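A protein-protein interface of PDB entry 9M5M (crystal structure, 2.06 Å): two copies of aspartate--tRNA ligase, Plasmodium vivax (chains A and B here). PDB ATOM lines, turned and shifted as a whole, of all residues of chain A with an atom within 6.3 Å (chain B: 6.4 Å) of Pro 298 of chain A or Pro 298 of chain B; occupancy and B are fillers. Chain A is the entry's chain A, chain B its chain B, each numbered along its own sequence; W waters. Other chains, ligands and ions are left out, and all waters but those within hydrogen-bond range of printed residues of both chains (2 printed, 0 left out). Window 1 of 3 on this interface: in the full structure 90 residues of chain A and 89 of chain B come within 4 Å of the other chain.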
ATOM      1  N   HIS A 247       1.175 -10.893  -8.987  1.00  0.00           N
ATOM      2  CA  HIS A 247       1.876 -10.934 -10.270  1.00  0.00           C
ATOM      3  C   HIS A 247       0.902 -11.479 -11.293  1.00  0.00           C
ATOM      4  O   HIS A 247       0.507 -12.651 -11.208  1.00  0.00           O
ATOM      5  CB  HIS A 247       3.129 -11.806 -10.208  1.00  0.00           C
ATOM      6  CG  HIS A 247       4.193 -11.258  -9.306  1.00  0.00           C
ATOM      7  ND1 HIS A 247       5.047 -10.250  -9.695  1.00  0.00           N
ATOM      8  CD2 HIS A 247       4.513 -11.547  -8.023  1.00  0.00           C
ATOM      9  CE1 HIS A 247       5.859  -9.949  -8.694  1.00  0.00           C
ATOM     10  NE2 HIS A 247       5.565 -10.729  -7.672  1.00  0.00           N
ATOM     11  N   THR A 248       0.520 -10.639 -12.251  1.00  0.00           N
ATOM     12  CA  THR A 248      -0.474 -10.989 -13.249  1.00  0.00           C
ATOM     13  C   THR A 248       0.137 -10.964 -14.649  1.00  0.00           C
ATOM     14  O   THR A 248       1.163 -10.313 -14.877  1.00  0.00           O
ATOM     15  CB  THR A 248      -1.672 -10.031 -13.153  1.00  0.00           C
ATOM     16  OG1 THR A 248      -1.252  -8.691 -13.441  1.00  0.00           O
ATOM     17  CG2 THR A 248      -2.275 -10.082 -11.746  1.00  0.00           C
ATOM     18  N   LYS A 250       1.376 -10.533 -18.531  1.00  0.00           N
ATOM     19  CA  LYS A 250       1.490  -9.493 -19.549  1.00  0.00           C
ATOM     20  C   LYS A 250       1.138  -9.989 -20.945  1.00  0.00           C
ATOM     21  O   LYS A 250       0.920  -9.166 -21.836  1.00  0.00           O
ATOM     22  CB  LYS A 250       2.907  -8.897 -19.571  1.00  0.00           C
ATOM     23  CG  LYS A 250       3.473  -8.588 -18.184  1.00  0.00           C
ATOM     24  CD  LYS A 250       2.490  -7.771 -17.358  1.00  0.00           C
ATOM     25  CE  LYS A 250       2.873  -7.740 -15.899  1.00  0.00           C
ATOM     26  NZ  LYS A 250       1.717  -7.286 -15.053  1.00  0.00           N
ATOM     27  N   ALA A 275       0.135  -6.543 -22.242  1.00  0.00           N
ATOM     28  CA  ALA A 275      -0.644  -5.722 -21.325  1.00  0.00           C
ATOM     29  C   ALA A 275      -0.147  -4.278 -21.302  1.00  0.00           C
ATOM     30  O   ALA A 275       1.043  -4.012 -21.098  1.00  0.00           O
ATOM     31  CB  ALA A 275      -0.592  -6.307 -19.911  1.00  0.00           C
ATOM     32  N   PRO A 278      -2.190  -3.899 -15.736  1.00  0.00           N
ATOM     33  CA  PRO A 278      -2.750  -5.125 -15.191  1.00  0.00           C
ATOM     34  C   PRO A 278      -4.142  -4.846 -14.618  1.00  0.00           C
ATOM     35  O   PRO A 278      -4.629  -5.581 -13.809  1.00  0.00           O
ATOM     36  CB  PRO A 278      -1.813  -5.404 -14.050  1.00  0.00           C
ATOM     37  CG  PRO A 278      -1.519  -4.049 -13.531  1.00  0.00           C
ATOM     38  CD  PRO A 278      -1.473  -3.142 -14.711  1.00  0.00           C
ATOM     39  N   GLU A 295       0.866  -4.412  -7.466  1.00  0.00           N
ATOM     40  CA  GLU A 295       1.784  -5.039  -8.406  1.00  0.00           C
ATOM     41  C   GLU A 295       2.829  -4.012  -8.811  1.00  0.00           C
ATOM     42  O   GLU A 295       2.514  -2.830  -8.967  1.00  0.00           O
ATOM     43  CB  GLU A 295       1.047  -5.575  -9.650  1.00  0.00           C
ATOM     44  CG  GLU A 295       1.958  -6.350 -10.600  1.00  0.00           C
ATOM     45  CD  GLU A 295       1.202  -7.260 -11.561  1.00  0.00           C
ATOM     46  OE1 GLU A 295      -0.057  -7.240 -11.551  1.00  0.00           O
ATOM     47  OE2 GLU A 295       1.878  -8.000 -12.330  1.00  0.00           O
ATOM     48  N   VAL A 296       4.077  -4.456  -8.947  1.00  0.00           N
ATOM     49  CA  VAL A 296       5.174  -3.646  -9.490  1.00  0.00           C
ATOM     50  C   VAL A 296       5.699  -4.416 -10.692  1.00  0.00           C
ATOM     51  O   VAL A 296       6.279  -5.497 -10.519  1.00  0.00           O
ATOM     52  CB  VAL A 296       6.287  -3.411  -8.455  1.00  0.00           C
ATOM     53  CG1 VAL A 296       7.473  -2.653  -9.081  1.00  0.00           C
ATOM     54  CG2 VAL A 296       5.740  -2.649  -7.258  1.00  0.00           C
ATOM     55  N   ALA A 297       5.464  -3.914 -11.902  1.00  0.00           N
ATOM     56  CA  ALA A 297       5.660  -4.792 -13.055  1.00  0.00           C
ATOM     57  C   ALA A 297       5.694  -3.956 -14.336  1.00  0.00           C
ATOM     58  O   ALA A 297       5.131  -2.855 -14.380  1.00  0.00           O
ATOM     59  CB  ALA A 297       4.550  -5.860 -13.141  1.00  0.00           C
ATOM     60  N   PRO A 298       6.337  -4.473 -15.389  1.00  0.00           N
ATOM     61  CA  PRO A 298       6.349  -3.772 -16.680  1.00  0.00           C
ATOM     62  C   PRO A 298       4.964  -3.665 -17.298  1.00  0.00           C
ATOM     63  O   PRO A 298       4.080  -4.494 -17.062  1.00  0.00           O
ATOM     64  CB  PRO A 298       7.254  -4.642 -17.564  1.00  0.00           C
ATOM     65  CG  PRO A 298       7.915  -5.614 -16.674  1.00  0.00           C
ATOM     66  CD  PRO A 298       7.074  -5.748 -15.444  1.00  0.00           C
ATOM     67  N   VAL A 299       4.793  -2.607 -18.092  1.00  0.00           N
ATOM     68  CA  VAL A 299       3.666  -2.438 -18.998  1.00  0.00           C
ATOM     69  C   VAL A 299       4.226  -1.910 -20.312  1.00  0.00           C
ATOM     70  O   VAL A 299       5.326  -1.334 -20.370  1.00  0.00           O
ATOM     71  CB  VAL A 299       2.573  -1.490 -18.448  1.00  0.00           C
ATOM     72  CG1 VAL A 299       1.977  -2.033 -17.144  1.00  0.00           C
ATOM     73  CG2 VAL A 299       3.121  -0.077 -18.239  1.00  0.00           C
ATOM     74  N   PHE A 300       3.440  -2.103 -21.371  1.00  0.00           N
ATOM     75  CA  PHE A 300       3.885  -1.930 -22.748  1.00  0.00           C
ATOM     76  C   PHE A 300       2.853  -1.128 -23.526  1.00  0.00           C
ATOM     77  O   PHE A 300       1.678  -1.510 -23.569  1.00  0.00           O
ATOM     78  CB  PHE A 300       4.095  -3.297 -23.414  1.00  0.00           C
ATOM     79  CG  PHE A 300       4.934  -4.244 -22.594  1.00  0.00           C
ATOM     80  CD1 PHE A 300       6.310  -4.318 -22.782  1.00  0.00           C
ATOM     81  CD2 PHE A 300       4.351  -5.053 -21.626  1.00  0.00           C
ATOM     82  CE1 PHE A 300       7.081  -5.180 -22.028  1.00  0.00           C
ATOM     83  CE2 PHE A 300       5.120  -5.923 -20.862  1.00  0.00           C
ATOM     84  CZ  PHE A 300       6.487  -5.987 -21.059  1.00  0.00           C
ATOM     85  N   GLU A 313       7.856   1.097 -23.043  1.00  0.00           N
ATOM     86  CA  GLU A 313       7.896   0.112 -21.981  1.00  0.00           C
ATOM     87  C   GLU A 313       8.306   0.830 -20.710  1.00  0.00           C
ATOM     88  O   GLU A 313       9.285   1.583 -20.716  1.00  0.00           O
ATOM     89  CB  GLU A 313       8.891  -1.015 -22.289  1.00  0.00           C
ATOM     90  CG  GLU A 313       9.145  -1.898 -21.072  1.00  0.00           C
ATOM     91  CD  GLU A 313      10.040  -3.102 -21.357  1.00  0.00           C
ATOM     92  OE1 GLU A 313      10.254  -3.886 -20.407  1.00  0.00           O
ATOM     93  OE2 GLU A 313      10.527  -3.265 -22.510  1.00  0.00           O
ATOM     94  N   TYR A 314       7.572   0.606 -19.625  1.00  0.00           N
ATOM     95  CA  TYR A 314       7.955   1.233 -18.366  1.00  0.00           C
ATOM     96  C   TYR A 314       7.425   0.377 -17.227  1.00  0.00           C
ATOM     97  O   TYR A 314       6.838  -0.681 -17.453  1.00  0.00           O
ATOM     98  CB  TYR A 314       7.480   2.699 -18.297  1.00  0.00           C
ATOM     99  CG  TYR A 314       5.972   2.919 -18.353  1.00  0.00           C
ATOM    100  CD1 TYR A 314       5.235   3.071 -17.189  1.00  0.00           C
ATOM    101  CD2 TYR A 314       5.293   2.983 -19.568  1.00  0.00           C
ATOM    102  CE1 TYR A 314       3.859   3.275 -17.225  1.00  0.00           C
ATOM    103  CE2 TYR A 314       3.903   3.183 -19.611  1.00  0.00           C
ATOM    104  CZ  TYR A 314       3.206   3.330 -18.432  1.00  0.00           C
ATOM    105  OH  TYR A 314       1.846   3.532 -18.437  1.00  0.00           O
ATOM    106  N   VAL A 315       7.678   0.814 -15.992  1.00  0.00           N
ATOM    107  CA  VAL A 315       7.297   0.072 -14.796  1.00  0.00           C
ATOM    108  C   VAL A 315       6.100   0.765 -14.169  1.00  0.00           C
ATOM    109  O   VAL A 315       6.144   1.974 -13.883  1.00  0.00           O
ATOM    110  CB  VAL A 315       8.455  -0.035 -13.794  1.00  0.00           C
ATOM    111  CG1 VAL A 315       7.967  -0.675 -12.455  1.00  0.00           C
ATOM    112  CG2 VAL A 315       9.602  -0.851 -14.398  1.00  0.00           C
ATOM    113  N   SER A 316       5.023   0.008 -13.983  1.00  0.00           N
ATOM    114  CA  SER A 316       3.807   0.503 -13.362  1.00  0.00           C
ATOM    115  C   SER A 316       3.720  -0.013 -11.934  1.00  0.00           C
ATOM    116  O   SER A 316       3.967  -1.199 -11.673  1.00  0.00           O
ATOM    117  CB  SER A 316       2.565   0.081 -14.146  1.00  0.00           C
ATOM    118  OG  SER A 316       1.394   0.708 -13.626  1.00  0.00           O
ATOM    119  N   HIS B 247      15.158  -2.460 -12.864  1.00  0.00           N
ATOM    120  CA  HIS B 247      14.103  -2.822 -13.809  1.00  0.00           C
ATOM    121  C   HIS B 247      14.669  -2.670 -15.205  1.00  0.00           C
ATOM    122  O   HIS B 247      15.039  -1.561 -15.605  1.00  0.00           O
ATOM    123  CB  HIS B 247      12.865  -1.938 -13.642  1.00  0.00           C
ATOM    124  CG  HIS B 247      12.199  -2.113 -12.321  1.00  0.00           C
ATOM    125  ND1 HIS B 247      11.348  -3.166 -12.052  1.00  0.00           N
ATOM    126  CD2 HIS B 247      12.269  -1.381 -11.185  1.00  0.00           C
ATOM    127  CE1 HIS B 247      10.928  -3.075 -10.803  1.00  0.00           C
ATOM    128  NE2 HIS B 247      11.470  -2.001 -10.256  1.00  0.00           N
ATOM    129  N   THR B 248      14.750  -3.775 -15.935  1.00  0.00           N
ATOM    130  CA  THR B 248      15.379  -3.818 -17.241  1.00  0.00           C
ATOM    131  C   THR B 248      14.353  -4.268 -18.270  1.00  0.00           C
ATOM    132  O   THR B 248      13.342  -4.883 -17.911  1.00  0.00           O
ATOM    133  CB  THR B 248      16.590  -4.764 -17.215  1.00  0.00           C
ATOM    134  OG1 THR B 248      16.146  -6.090 -16.899  1.00  0.00           O
ATOM    135  CG2 THR B 248      17.587  -4.296 -16.139  1.00  0.00           C
ATOM    136  N   LYS B 250      11.941  -5.817 -21.226  1.00  0.00           N
ATOM    137  CA  LYS B 250      11.510  -7.116 -21.725  1.00  0.00           C
ATOM    138  C   LYS B 250      11.329  -7.132 -23.232  1.00  0.00           C
ATOM    139  O   LYS B 250      11.191  -8.221 -23.809  1.00  0.00           O
ATOM    140  CB  LYS B 250      10.203  -7.548 -21.043  1.00  0.00           C
ATOM    141  CG  LYS B 250      10.215  -7.371 -19.527  1.00  0.00           C
ATOM    142  CD  LYS B 250      11.437  -8.032 -18.854  1.00  0.00           C
ATOM    143  CE  LYS B 250      11.626  -7.456 -17.438  1.00  0.00           C
ATOM    144  NZ  LYS B 250      12.960  -7.751 -16.822  1.00  0.00           N
ATOM    145  N   ALA B 275      11.933 -10.883 -23.650  1.00  0.00           N
ATOM    146  CA  ALA B 275      13.012 -11.405 -22.860  1.00  0.00           C
ATOM    147  C   ALA B 275      12.713 -12.713 -22.163  1.00  0.00           C
ATOM    148  O   ALA B 275      11.671 -12.897 -21.605  1.00  0.00           O
ATOM    149  CB  ALA B 275      13.451 -10.381 -21.845  1.00  0.00           C
ATOM    150  N   PRO B 278      16.617 -11.518 -17.750  1.00  0.00           N
ATOM    151  CA  PRO B 278      17.237 -10.207 -17.799  1.00  0.00           C
ATOM    152  C   PRO B 278      18.743 -10.341 -17.688  1.00  0.00           C
ATOM    153  O   PRO B 278      19.388  -9.383 -17.377  1.00  0.00           O
ATOM    154  CB  PRO B 278      16.696  -9.546 -16.560  1.00  0.00           C
ATOM    155  CG  PRO B 278      16.566 -10.657 -15.604  1.00  0.00           C
ATOM    156  CD  PRO B 278      16.149 -11.840 -16.403  1.00  0.00           C
ATOM    157  N   GLU B 295      16.322  -8.173  -9.580  1.00  0.00           N
ATOM    158  CA  GLU B 295      15.105  -7.830 -10.305  1.00  0.00           C
ATOM    159  C   GLU B 295      14.052  -8.890  -9.993  1.00  0.00           C
ATOM    160  O   GLU B 295      14.368 -10.078  -9.853  1.00  0.00           O
ATOM    161  CB  GLU B 295      15.362  -7.729 -11.817  1.00  0.00           C
ATOM    162  CG  GLU B 295      14.163  -7.151 -12.615  1.00  0.00           C
ATOM    163  CD  GLU B 295      14.506  -6.760 -14.043  1.00  0.00           C
ATOM    164  OE1 GLU B 295      13.610  -6.346 -14.818  1.00  0.00           O
ATOM    165  OE2 GLU B 295      15.705  -6.872 -14.401  1.00  0.00           O
ATOM    166  N   VAL B 296      12.812  -8.454  -9.819  1.00  0.00           N
ATOM    167  CA  VAL B 296      11.666  -9.350  -9.683  1.00  0.00           C
ATOM    168  C   VAL B 296      10.720  -8.974 -10.808  1.00  0.00           C
ATOM    169  O   VAL B 296      10.094  -7.905 -10.755  1.00  0.00           O
ATOM    170  CB  VAL B 296      10.976  -9.223  -8.314  1.00  0.00           C
ATOM    171  CG1 VAL B 296       9.729 -10.098  -8.276  1.00  0.00           C
ATOM    172  CG2 VAL B 296      11.929  -9.611  -7.170  1.00  0.00           C
ATOM    173  N   ALA B 297      10.625  -9.816 -11.841  1.00  0.00           N
ATOM    174  CA  ALA B 297       9.929  -9.340 -13.032  1.00  0.00           C
ATOM    175  C   ALA B 297       9.535 -10.524 -13.895  1.00  0.00           C
ATOM    176  O   ALA B 297      10.107 -11.616 -13.756  1.00  0.00           O
ATOM    177  CB  ALA B 297      10.812  -8.353 -13.832  1.00  0.00           C
ATOM    178  N   PRO B 298       8.565 -10.336 -14.800  1.00  0.00           N
ATOM    179  CA  PRO B 298       8.202 -11.418 -15.724  1.00  0.00           C
ATOM    180  C   PRO B 298       9.316 -11.753 -16.697  1.00  0.00           C
ATOM    181  O   PRO B 298      10.135 -10.907 -17.070  1.00  0.00           O
ATOM    182  CB  PRO B 298       6.990 -10.861 -16.490  1.00  0.00           C
ATOM    183  CG  PRO B 298       6.608  -9.586 -15.839  1.00  0.00           C
ATOM    184  CD  PRO B 298       7.702  -9.149 -14.938  1.00  0.00           C
ATOM    185  N   VAL B 299       9.313 -13.021 -17.111  1.00  0.00           N
ATOM    186  CA  VAL B 299      10.033 -13.516 -18.272  1.00  0.00           C
ATOM    187  C   VAL B 299       9.052 -14.358 -19.088  1.00  0.00           C
ATOM    188  O   VAL B 299       8.034 -14.849 -18.576  1.00  0.00           O
ATOM    189  CB  VAL B 299      11.287 -14.345 -17.891  1.00  0.00           C
ATOM    190  CG1 VAL B 299      12.262 -13.508 -17.070  1.00  0.00           C
ATOM    191  CG2 VAL B 299      10.879 -15.582 -17.098  1.00  0.00           C
ATOM    192  N   PHE B 300       9.385 -14.525 -20.375  1.00  0.00           N
ATOM    193  CA  PHE B 300       8.515 -15.141 -21.370  1.00  0.00           C
ATOM    194  C   PHE B 300       9.321 -16.144 -22.176  1.00  0.00           C
ATOM    195  O   PHE B 300      10.409 -15.815 -22.670  1.00  0.00           O
ATOM    196  CB  PHE B 300       7.916 -14.088 -22.314  1.00  0.00           C
ATOM    197  CG  PHE B 300       7.399 -12.859 -21.606  1.00  0.00           C
ATOM    198  CD1 PHE B 300       6.072 -12.773 -21.221  1.00  0.00           C
ATOM    199  CD2 PHE B 300       8.242 -11.805 -21.309  1.00  0.00           C
ATOM    200  CE1 PHE B 300       5.589 -11.649 -20.570  1.00  0.00           C
ATOM    201  CE2 PHE B 300       7.771 -10.682 -20.658  1.00  0.00           C
ATOM    202  CZ  PHE B 300       6.443 -10.607 -20.279  1.00  0.00           C
ATOM    203  N   GLU B 313       4.910 -17.925 -19.400  1.00  0.00           N
ATOM    204  CA  GLU B 313       5.227 -16.677 -18.728  1.00  0.00           C
ATOM    205  C   GLU B 313       5.299 -16.945 -17.233  1.00  0.00           C
ATOM    206  O   GLU B 313       4.441 -17.646 -16.683  1.00  0.00           O
ATOM    207  CB  GLU B 313       4.179 -15.604 -19.040  1.00  0.00           C
ATOM    208  CG  GLU B 313       4.477 -14.268 -18.386  1.00  0.00           C
ATOM    209  CD  GLU B 313       3.331 -13.289 -18.544  1.00  0.00           C
ATOM    210  OE1 GLU B 313       3.378 -12.231 -17.878  1.00  0.00           O
ATOM    211  OE2 GLU B 313       2.393 -13.582 -19.333  1.00  0.00           O
ATOM    212  N   TYR B 314       6.319 -16.409 -16.573  1.00  0.00           N
ATOM    213  CA  TYR B 314       6.361 -16.556 -15.121  1.00  0.00           C
ATOM    214  C   TYR B 314       7.209 -15.428 -14.554  1.00  0.00           C
ATOM    215  O   TYR B 314       7.669 -14.550 -15.287  1.00  0.00           O
ATOM    216  CB  TYR B 314       6.867 -17.948 -14.717  1.00  0.00           C
ATOM    217  CG  TYR B 314       8.250 -18.245 -15.224  1.00  0.00           C
ATOM    218  CD1 TYR B 314       9.367 -18.041 -14.410  1.00  0.00           C
ATOM    219  CD2 TYR B 314       8.447 -18.698 -16.521  1.00  0.00           C
ATOM    220  CE1 TYR B 314      10.643 -18.301 -14.872  1.00  0.00           C
ATOM    221  CE2 TYR B 314       9.725 -18.960 -16.997  1.00  0.00           C
ATOM    222  CZ  TYR B 314      10.812 -18.757 -16.169  1.00  0.00           C
ATOM    223  OH  TYR B 314      12.082 -19.006 -16.634  1.00  0.00           O
ATOM    224  N   VAL B 315       7.365 -15.421 -13.235  1.00  0.00           N
ATOM    225  CA  VAL B 315       8.101 -14.363 -12.547  1.00  0.00           C
ATOM    226  C   VAL B 315       9.474 -14.901 -12.179  1.00  0.00           C
ATOM    227  O   VAL B 315       9.582 -15.915 -11.477  1.00  0.00           O
ATOM    228  CB  VAL B 315       7.347 -13.857 -11.306  1.00  0.00           C
ATOM    229  CG1 VAL B 315       8.190 -12.851 -10.536  1.00  0.00           C
ATOM    230  CG2 VAL B 315       6.027 -13.230 -11.725  1.00  0.00           C
ATOM    231  N   SER B 316      10.518 -14.231 -12.668  1.00  0.00           N
ATOM    232  CA  SER B 316      11.898 -14.567 -12.344  1.00  0.00           C
ATOM    233  C   SER B 316      12.406 -13.645 -11.244  1.00  0.00           C
ATOM    234  O   SER B 316      12.182 -12.424 -11.286  1.00  0.00           O
ATOM    235  CB  SER B 316      12.799 -14.454 -13.579  1.00  0.00           C
ATOM    236  OG  SER B 316      14.084 -15.006 -13.318  1.00  0.00           O
HETATM  237  O   HOH W   1       9.122  -5.564 -12.555  1.00  0.00           O
HETATM  238  O   HOH W   2       8.292  -6.590  -8.907  1.00  0.00           O
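Water W2 lies within hydrogen-bond range of the backbone carbonyl oxygen (O) of Val 296 of chain A (2.8 Å) and the backbone carbonyl oxygen (O) of Val 296 of chain B (2.9 Å). Water W1 lies within hydrogen-bond range of the backbone carbonyl oxygen of Val 296 of chain B, a ring nitrogen (ND1) of His 247 of chain B and the backbone carbonyl oxygen of Val 296 of chain A.
Among the printed residues, pairs that only touch across the chains: Pro 298 of chain A with Pro 298 of chain B, Val 315 of chain A with His 247 of chain B, His 247 of chain A with Val 315 of chain B, Val 296 of chain A with His 247 of chain B, His 247 of chain A with Val 296 of chain B and Lys 250 of chain A with Phe 300 of chain B.
Hydrophobic or aromatic side chains of chain A within 4 Å of the printed part of chain B: His 247, Val 296, Pro 298 and Val 315. Along chain B the printed residues that touch a printed residue of chain A span positions 247 to 315. Among the printed residues, 8 pairs touch across the chains. Among the printed residues, no Asp or Glu carboxylate lies within 4 Å of a Lys or Arg side-chain nitrogen of the other chain.
The backbone NH of Lys 250 of chain A sits at hydrogen-bond distance from the side-chain carboxylate of Glu 313 of chain B, at 2.7 Å. OE1 of Glu 313 of chain A is in hydrogen-bond range of N of Lys 250 of chain B, at 2.7 Å.
The backbone carbonyl oxygen (O) of Lys 250 of chain A lies within hydrogen-bond range of the backbone NH (N) of Ala 275 of chain A, at 2.8 Å. NZ of Lys 250 of chain A is in salt-bridge range of OE2 of Glu 295 of chain A (2.8 Å). The backbone carbonyl oxygen of Thr 248 of chain B lies within hydrogen-bond range of the side-chain amino group of Lys 250 of chain B (3.1 Å). The backbone carbonyl oxygen of Lys 250 of chain B lies within hydrogen-bond range of the backbone NH of Ala 275 of chain B, at 2.8 Å. The side-chain amino group (NZ) of Lys 250 of chain B lies within salt-bridge range of the side-chain carboxylate (OE1) of Glu 295 of chain B (2.5 Å). The backbone carbonyl oxygen (O) of Ala 275 of chain B is in hydrogen-bond range of the backbone NH (N) of Phe 300 of chain B.
Of chain B, only Pro 298 (3.5 Å) comes within 4 Å of Pro 298 of chain A. Of chain A, only Pro 298 comes within 4 Å of Pro 298 of chain B. Printed residues of chain B within 4 Å of Val 315 of chain A: His 247. Printed residues of chain A within 4 Å of Lys 250 of chain B: Glu 313. Printed residues of chain A within 4 Å of His 247 of chain B: Val 296 and Val 315. Of the printed residues of chain A, Phe 300 of chain B touches Lys 250 (3.97 Å). The nearest residue of chain B that does not touch Pro 298 of chain A is Lys 250 of chain B (4.1 Å). The nearest printed residue of chain A that does not touch Glu 313 of chain B is Thr 248 of chain A (4.2 Å).
His 247 of chain A touches Val 296 of chain B, and with the chains exchanged Val 296 of chain A touches His 247 of chain B. His 247 of chain A touches Val 315 of chain B, and with the chains exchanged Val 315 of chain A touches His 247 of chain B. Lys 250 of chain A touches Phe 300 of chain B, but with the chains exchanged Phe 300 of chain A does not touch Lys 250 of chain B (4.03 Å). Lys 250 of chain A touches Glu 313 of chain B, and with the chains exchanged Glu 313 of chain A touches Lys 250 of chain B. 15 positions are printed for both chains.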
